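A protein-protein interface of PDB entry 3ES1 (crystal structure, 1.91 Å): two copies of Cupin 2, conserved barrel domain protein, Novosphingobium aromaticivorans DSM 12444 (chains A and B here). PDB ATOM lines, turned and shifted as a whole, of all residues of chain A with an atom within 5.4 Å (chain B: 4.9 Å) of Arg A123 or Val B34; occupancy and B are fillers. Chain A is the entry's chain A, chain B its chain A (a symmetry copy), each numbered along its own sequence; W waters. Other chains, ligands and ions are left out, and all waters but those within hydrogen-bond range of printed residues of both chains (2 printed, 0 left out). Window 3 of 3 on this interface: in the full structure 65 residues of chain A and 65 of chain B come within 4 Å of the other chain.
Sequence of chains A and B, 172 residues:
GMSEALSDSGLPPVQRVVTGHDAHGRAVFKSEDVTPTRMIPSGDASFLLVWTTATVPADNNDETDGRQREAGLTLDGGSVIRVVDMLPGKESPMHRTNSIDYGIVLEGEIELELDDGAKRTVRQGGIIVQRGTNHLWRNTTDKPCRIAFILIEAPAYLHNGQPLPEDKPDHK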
ATOM      1  N   VAL A 105      13.336 -17.187 -17.051  1.00  0.00           N
ATOM      2  CA  VAL A 105      12.080 -17.954 -16.957  1.00  0.00           C
ATOM      3  C   VAL A 105      11.127 -17.503 -18.078  1.00  0.00           C
ATOM      4  O   VAL A 105      10.584 -16.379 -18.040  1.00  0.00           O
ATOM      5  CB  VAL A 105      11.425 -17.888 -15.540  1.00  0.00           C
ATOM      6  CG1 VAL A 105      10.245 -18.852 -15.449  1.00  0.00           C
ATOM      7  CG2 VAL A 105      12.434 -18.180 -14.412  1.00  0.00           C
ATOM      8  N   GLY A 108       5.820 -20.094 -16.956  1.00  0.00           N
ATOM      9  CA  GLY A 108       5.630 -20.700 -15.663  1.00  0.00           C
ATOM     10  C   GLY A 108       6.522 -20.078 -14.604  1.00  0.00           C
ATOM     11  O   GLY A 108       7.052 -18.998 -14.769  1.00  0.00           O
ATOM     12  N   GLU A 109       6.625 -20.788 -13.495  1.00  0.00           N
ATOM     13  CA  GLU A 109       7.534 -20.429 -12.434  1.00  0.00           C
ATOM     14  C   GLU A 109       8.192 -21.631 -11.821  1.00  0.00           C
ATOM     15  O   GLU A 109       7.731 -22.774 -11.925  1.00  0.00           O
ATOM     16  CB  GLU A 109       6.875 -19.574 -11.373  1.00  0.00           C
ATOM     17  CG  GLU A 109       5.702 -20.174 -10.668  1.00  0.00           C
ATOM     18  CD  GLU A 109       5.008 -19.133  -9.795  1.00  0.00           C
ATOM     19  OE1 GLU A 109       4.740 -18.009 -10.270  1.00  0.00           O
ATOM     20  OE2 GLU A 109       4.764 -19.417  -8.629  1.00  0.00           O
ATOM     21  N   ILE A 110       9.292 -21.309 -11.175  1.00  0.00           N
ATOM     22  CA  ILE A 110      10.271 -22.287 -10.687  1.00  0.00           C
ATOM     23  C   ILE A 110      10.800 -21.966  -9.274  1.00  0.00           C
ATOM     24  O   ILE A 110      10.979 -20.810  -8.888  1.00  0.00           O
ATOM     25  CB  ILE A 110      11.484 -22.407 -11.657  1.00  0.00           C
ATOM     26  CG1 ILE A 110      12.139 -23.782 -11.504  1.00  0.00           C
ATOM     27  CG2 ILE A 110      12.520 -21.315 -11.377  1.00  0.00           C
ATOM     28  CD1 ILE A 110      11.267 -24.983 -12.043  1.00  0.00           C
ATOM     29  N   THR A 121      11.256 -18.645  -5.113  1.00  0.00           N
ATOM     30  CA  THR A 121      10.564 -18.773  -6.375  1.00  0.00           C
ATOM     31  C   THR A 121      10.998 -17.682  -7.342  1.00  0.00           C
ATOM     32  O   THR A 121      11.107 -16.510  -6.981  1.00  0.00           O
ATOM     33  CB  THR A 121       9.052 -18.778  -6.183  1.00  0.00           C
ATOM     34  OG1 THR A 121       8.653 -20.034  -5.581  1.00  0.00           O
ATOM     35  CG2 THR A 121       8.339 -18.594  -7.509  1.00  0.00           C
ATOM     36  N   VAL A 122      11.290 -18.099  -8.572  1.00  0.00           N
ATOM     37  CA  VAL A 122      11.546 -17.170  -9.660  1.00  0.00           C
ATOM     38  C   VAL A 122      10.368 -17.239 -10.605  1.00  0.00           C
ATOM     39  O   VAL A 122      10.055 -18.268 -11.194  1.00  0.00           O
ATOM     40  CB  VAL A 122      12.827 -17.452 -10.438  1.00  0.00           C
ATOM     41  CG1 VAL A 122      13.113 -16.305 -11.410  1.00  0.00           C
ATOM     42  CG2 VAL A 122      14.009 -17.638  -9.476  1.00  0.00           C
ATOM     43  N   ARG A 123       9.698 -16.108 -10.683  1.00  0.00           N
ATOM     44  CA  ARG A 123       8.485 -16.000 -11.438  1.00  0.00           C
ATOM     45  C   ARG A 123       8.766 -15.823 -12.928  1.00  0.00           C
ATOM     46  O   ARG A 123       9.901 -15.612 -13.367  1.00  0.00           O
ATOM     47  CB  ARG A 123       7.639 -14.824 -10.896  1.00  0.00           C
ATOM     48  CG  ARG A 123       7.199 -14.973  -9.468  1.00  0.00           C
ATOM     49  CD  ARG A 123       6.439 -13.699  -9.000  1.00  0.00           C
ATOM     50  NE  ARG A 123       7.295 -12.525  -9.045  1.00  0.00           N
ATOM     51  CZ  ARG A 123       8.110 -12.166  -8.051  1.00  0.00           C
ATOM     52  NH1 ARG A 123       8.183 -12.888  -6.945  1.00  0.00           N
ATOM     53  NH2 ARG A 123       8.897 -11.118  -8.176  1.00  0.00           N
ATOM     54  N   GLN A 124       7.709 -15.978 -13.691  1.00  0.00           N
ATOM     55  CA  GLN A 124       7.796 -15.830 -15.142  1.00  0.00           C
ATOM     56  C   GLN A 124       8.386 -14.472 -15.482  1.00  0.00           C
ATOM     57  O   GLN A 124       8.054 -13.457 -14.867  1.00  0.00           O
ATOM     58  CB  GLN A 124       6.434 -16.053 -15.796  1.00  0.00           C
ATOM     59  CG  GLN A 124       6.479 -16.115 -17.301  1.00  0.00           C
ATOM     60  CD  GLN A 124       5.147 -16.490 -17.919  1.00  0.00           C
ATOM     61  OE1 GLN A 124       4.470 -17.474 -17.521  1.00  0.00           O
ATOM     62  NE2 GLN A 124       4.730 -15.677 -18.886  1.00  0.00           N
ATOM     63  N   GLY A 125       9.328 -14.462 -16.425  1.00  0.00           N
ATOM     64  CA  GLY A 125      10.046 -13.262 -16.816  1.00  0.00           C
ATOM     65  C   GLY A 125      11.235 -12.918 -15.961  1.00  0.00           C
ATOM     66  O   GLY A 125      11.988 -11.993 -16.265  1.00  0.00           O
ATOM     67  N   GLY A 126      11.403 -13.683 -14.882  1.00  0.00           N
ATOM     68  CA  GLY A 126      12.509 -13.520 -13.953  1.00  0.00           C
ATOM     69  C   GLY A 126      13.844 -14.053 -14.472  1.00  0.00           C
ATOM     70  O   GLY A 126      13.897 -14.990 -15.304  1.00  0.00           O
ATOM     71  N   GLU B   4      10.212  -0.675  -8.316  1.00  0.00           N
ATOM     72  CA  GLU B   4       8.941  -1.452  -8.546  1.00  0.00           C
ATOM     73  C   GLU B   4       7.829  -0.522  -9.014  1.00  0.00           C
ATOM     74  O   GLU B   4       7.009   0.020  -8.261  1.00  0.00           O
ATOM     75  CB  GLU B   4       8.522  -2.268  -7.319  1.00  0.00           C
ATOM     76  CG  GLU B   4       9.450  -3.449  -6.997  1.00  0.00           C
ATOM     77  CD  GLU B   4      10.451  -3.167  -5.890  1.00  0.00           C
ATOM     78  OE1 GLU B   4      11.158  -2.133  -5.952  1.00  0.00           O
ATOM     79  OE2 GLU B   4      10.552  -3.999  -4.961  1.00  0.00           O
ATOM     80  N   PRO B  13       7.967  -5.058 -14.586  1.00  0.00           N
ATOM     81  CA  PRO B  13       9.383  -4.986 -14.206  1.00  0.00           C
ATOM     82  C   PRO B  13       9.956  -6.374 -14.139  1.00  0.00           C
ATOM     83  O   PRO B  13       9.242  -7.373 -14.135  1.00  0.00           O
ATOM     84  CB  PRO B  13       9.371  -4.343 -12.816  1.00  0.00           C
ATOM     85  CG  PRO B  13       7.985  -4.596 -12.262  1.00  0.00           C
ATOM     86  CD  PRO B  13       7.060  -4.698 -13.481  1.00  0.00           C
ATOM     87  N   VAL B  14      11.268  -6.419 -14.056  1.00  0.00           N
ATOM     88  CA  VAL B  14      12.017  -7.676 -14.115  1.00  0.00           C
ATOM     89  C   VAL B  14      12.608  -8.072 -12.746  1.00  0.00           C
ATOM     90  O   VAL B  14      13.320  -7.324 -12.130  1.00  0.00           O
ATOM     91  CB  VAL B  14      13.157  -7.534 -15.151  1.00  0.00           C
ATOM     92  CG1 VAL B  14      14.029  -8.828 -15.225  1.00  0.00           C
ATOM     93  CG2 VAL B  14      12.603  -7.096 -16.539  1.00  0.00           C
ATOM     94  N   GLN B  15      12.267  -9.269 -12.297  1.00  0.00           N
ATOM     95  CA  GLN B  15      12.879  -9.893 -11.112  1.00  0.00           C
ATOM     96  C   GLN B  15      14.243 -10.441 -11.460  1.00  0.00           C
ATOM     97  O   GLN B  15      14.403 -11.192 -12.433  1.00  0.00           O
ATOM     98  CB  GLN B  15      11.973 -11.047 -10.593  1.00  0.00           C
ATOM     99  CG  GLN B  15      12.511 -11.822  -9.377  1.00  0.00           C
ATOM    100  CD  GLN B  15      11.709 -13.065  -9.110  1.00  0.00           C
ATOM    101  OE1 GLN B  15      10.987 -13.567 -10.008  1.00  0.00           O
ATOM    102  NE2 GLN B  15      11.852 -13.611  -7.898  1.00  0.00           N
ATOM    103  N   GLU B  32      18.126  -9.960  -4.387  1.00  0.00           N
ATOM    104  CA  GLU B  32      16.907 -10.050  -5.198  1.00  0.00           C
ATOM    105  C   GLU B  32      16.269  -8.696  -5.344  1.00  0.00           C
ATOM    106  O   GLU B  32      16.214  -7.921  -4.388  1.00  0.00           O
ATOM    107  CB  GLU B  32      15.925 -11.020  -4.567  1.00  0.00           C
ATOM    108  CG  GLU B  32      14.577 -11.173  -5.298  1.00  0.00           C
ATOM    109  CD  GLU B  32      13.634 -12.161  -4.620  1.00  0.00           C
ATOM    110  OE1 GLU B  32      13.875 -12.562  -3.460  1.00  0.00           O
ATOM    111  OE2 GLU B  32      12.590 -12.488  -5.226  1.00  0.00           O
ATOM    112  N   ASP B  33      15.810  -8.406  -6.547  1.00  0.00           N
ATOM    113  CA  ASP B  33      15.187  -7.107  -6.833  1.00  0.00           C
ATOM    114  C   ASP B  33      14.203  -7.245  -7.954  1.00  0.00           C
ATOM    115  O   ASP B  33      14.335  -8.119  -8.774  1.00  0.00           O
ATOM    116  CB  ASP B  33      16.212  -6.015  -7.204  1.00  0.00           C
ATOM    117  CG  ASP B  33      17.014  -6.328  -8.453  1.00  0.00           C
ATOM    118  OD1 ASP B  33      18.067  -6.963  -8.330  1.00  0.00           O
ATOM    119  OD2 ASP B  33      16.613  -5.914  -9.564  1.00  0.00           O
ATOM    120  N   VAL B  34      13.230  -6.332  -7.981  1.00  0.00           N
ATOM    121  CA  VAL B  34      12.283  -6.245  -9.093  1.00  0.00           C
ATOM    122  C   VAL B  34      12.367  -4.815  -9.606  1.00  0.00           C
ATOM    123  O   VAL B  34      12.025  -3.882  -8.881  1.00  0.00           O
ATOM    124  CB  VAL B  34      10.822  -6.572  -8.635  1.00  0.00           C
ATOM    125  CG1 VAL B  34       9.789  -6.300  -9.744  1.00  0.00           C
ATOM    126  CG2 VAL B  34      10.736  -8.024  -8.113  1.00  0.00           C
ATOM    127  N   THR B  35      12.822  -4.672 -10.856  1.00  0.00           N
ATOM    128  CA  THR B  35      13.233  -3.388 -11.439  1.00  0.00           C
ATOM    129  C   THR B  35      12.682  -3.174 -12.866  1.00  0.00           C
ATOM    130  O   THR B  35      12.749  -4.067 -13.692  1.00  0.00           O
ATOM    131  CB  THR B  35      14.779  -3.330 -11.531  1.00  0.00           C
ATOM    132  OG1 THR B  35      15.319  -3.576 -10.230  1.00  0.00           O
ATOM    133  CG2 THR B  35      15.267  -1.956 -11.950  1.00  0.00           C
ATOM    134  N   PRO B  36      12.134  -1.978 -13.154  1.00  0.00           N
ATOM    135  CA  PRO B  36      11.620  -1.699 -14.494  1.00  0.00           C
ATOM    136  C   PRO B  36      12.696  -1.488 -15.533  1.00  0.00           C
ATOM    137  O   PRO B  36      13.776  -1.027 -15.219  1.00  0.00           O
ATOM    138  CB  PRO B  36      10.828  -0.399 -14.283  1.00  0.00           C
ATOM    139  CG  PRO B  36      11.575   0.299 -13.175  1.00  0.00           C
ATOM    140  CD  PRO B  36      11.929  -0.835 -12.239  1.00  0.00           C
HETATM  141  O   HOH W   1       9.898 -11.083 -13.394  1.00  0.00           O
HETATM  142  O   HOH W   2      10.645 -10.580  -5.835  1.00  0.00           O
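Val B34 touches just one residue of chain A: Arg A123. Printed residues of chain B within 4 Å of Thr A121: Gln B15 (3.1 Å). Of the printed residues of chain A, Gln B15 touches Thr A121, Val A122, Arg A123 and Gly A126. Printed residues of chain B within 4 Å of Val A122: Gln B15. Printed residues of chain B within 4 Å of Gly A126: Gln B15 (3.4 Å). Glu B32 touches none of the printed residues of chain A. The nearest printed residue of chain A that does not touch Val B34 is Gly A126 (8.2 Å). The nearest printed residue of chain B that does not touch Thr A121 is Glu B32 (4.6 Å).
Val A122 touches Gln B15 (CA to OE1, 3.7 Å). CG2 of Val B34 touches NH2 of Arg A123 (3.6 Å). CG1 of Val B14 touches O of Gly A125 (3.9 Å). Gln B15 touches Gly A126.
The backbone carbonyl oxygen of Thr A121 sits at hydrogen-bond distance from the side-chain amide nitrogen of Gln B15, 3.1 Å away. OE1 of Gln B15 is in hydrogen-bond range of N of Arg A123 (2.9 Å).
No position is printed for both chains. Of the 6 pairs that touch across the chains among the printed residues, none has its exchanged pair printed and touching as well.
Hydrophobic or aromatic side chains of chain B that line the printed part of chain A: Val B14 and Val B34. Of the 10 printed residues of chain A, 5 touch a printed residue of chain B. Among the printed residues, 6 pairs touch across the chains.
The backbone carbonyl oxygen of Val A105 lies within hydrogen-bond range of the backbone NH of Gly A125 (2.8 Å). O of Gly A126 sits at hydrogen-bond distance from N of Val A105, at 2.9 Å. O of Ile A110 sits at hydrogen-bond distance from N of Val A122 (2.7 Å). O of Thr B35 is in hydrogen-bond range of N of Val B14, at 2.8 Å. NE2 of Gln B15 is in hydrogen-bond range of OE2 of Glu B32 (3.0 Å).
Water W2 bridges the side-chain carboxylate (OE2) of Glu B32 (2.8 Å) and the guanidinium group (NH2) of Arg A123 (3.0 Å). Water W1 lies within hydrogen-bond range of the backbone NH of Gln B15 (3.2 Å), the backbone carbonyl oxygen of Gln A124 (3.3 Å) and the backbone NH of Gly A126 (3.4 Å).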
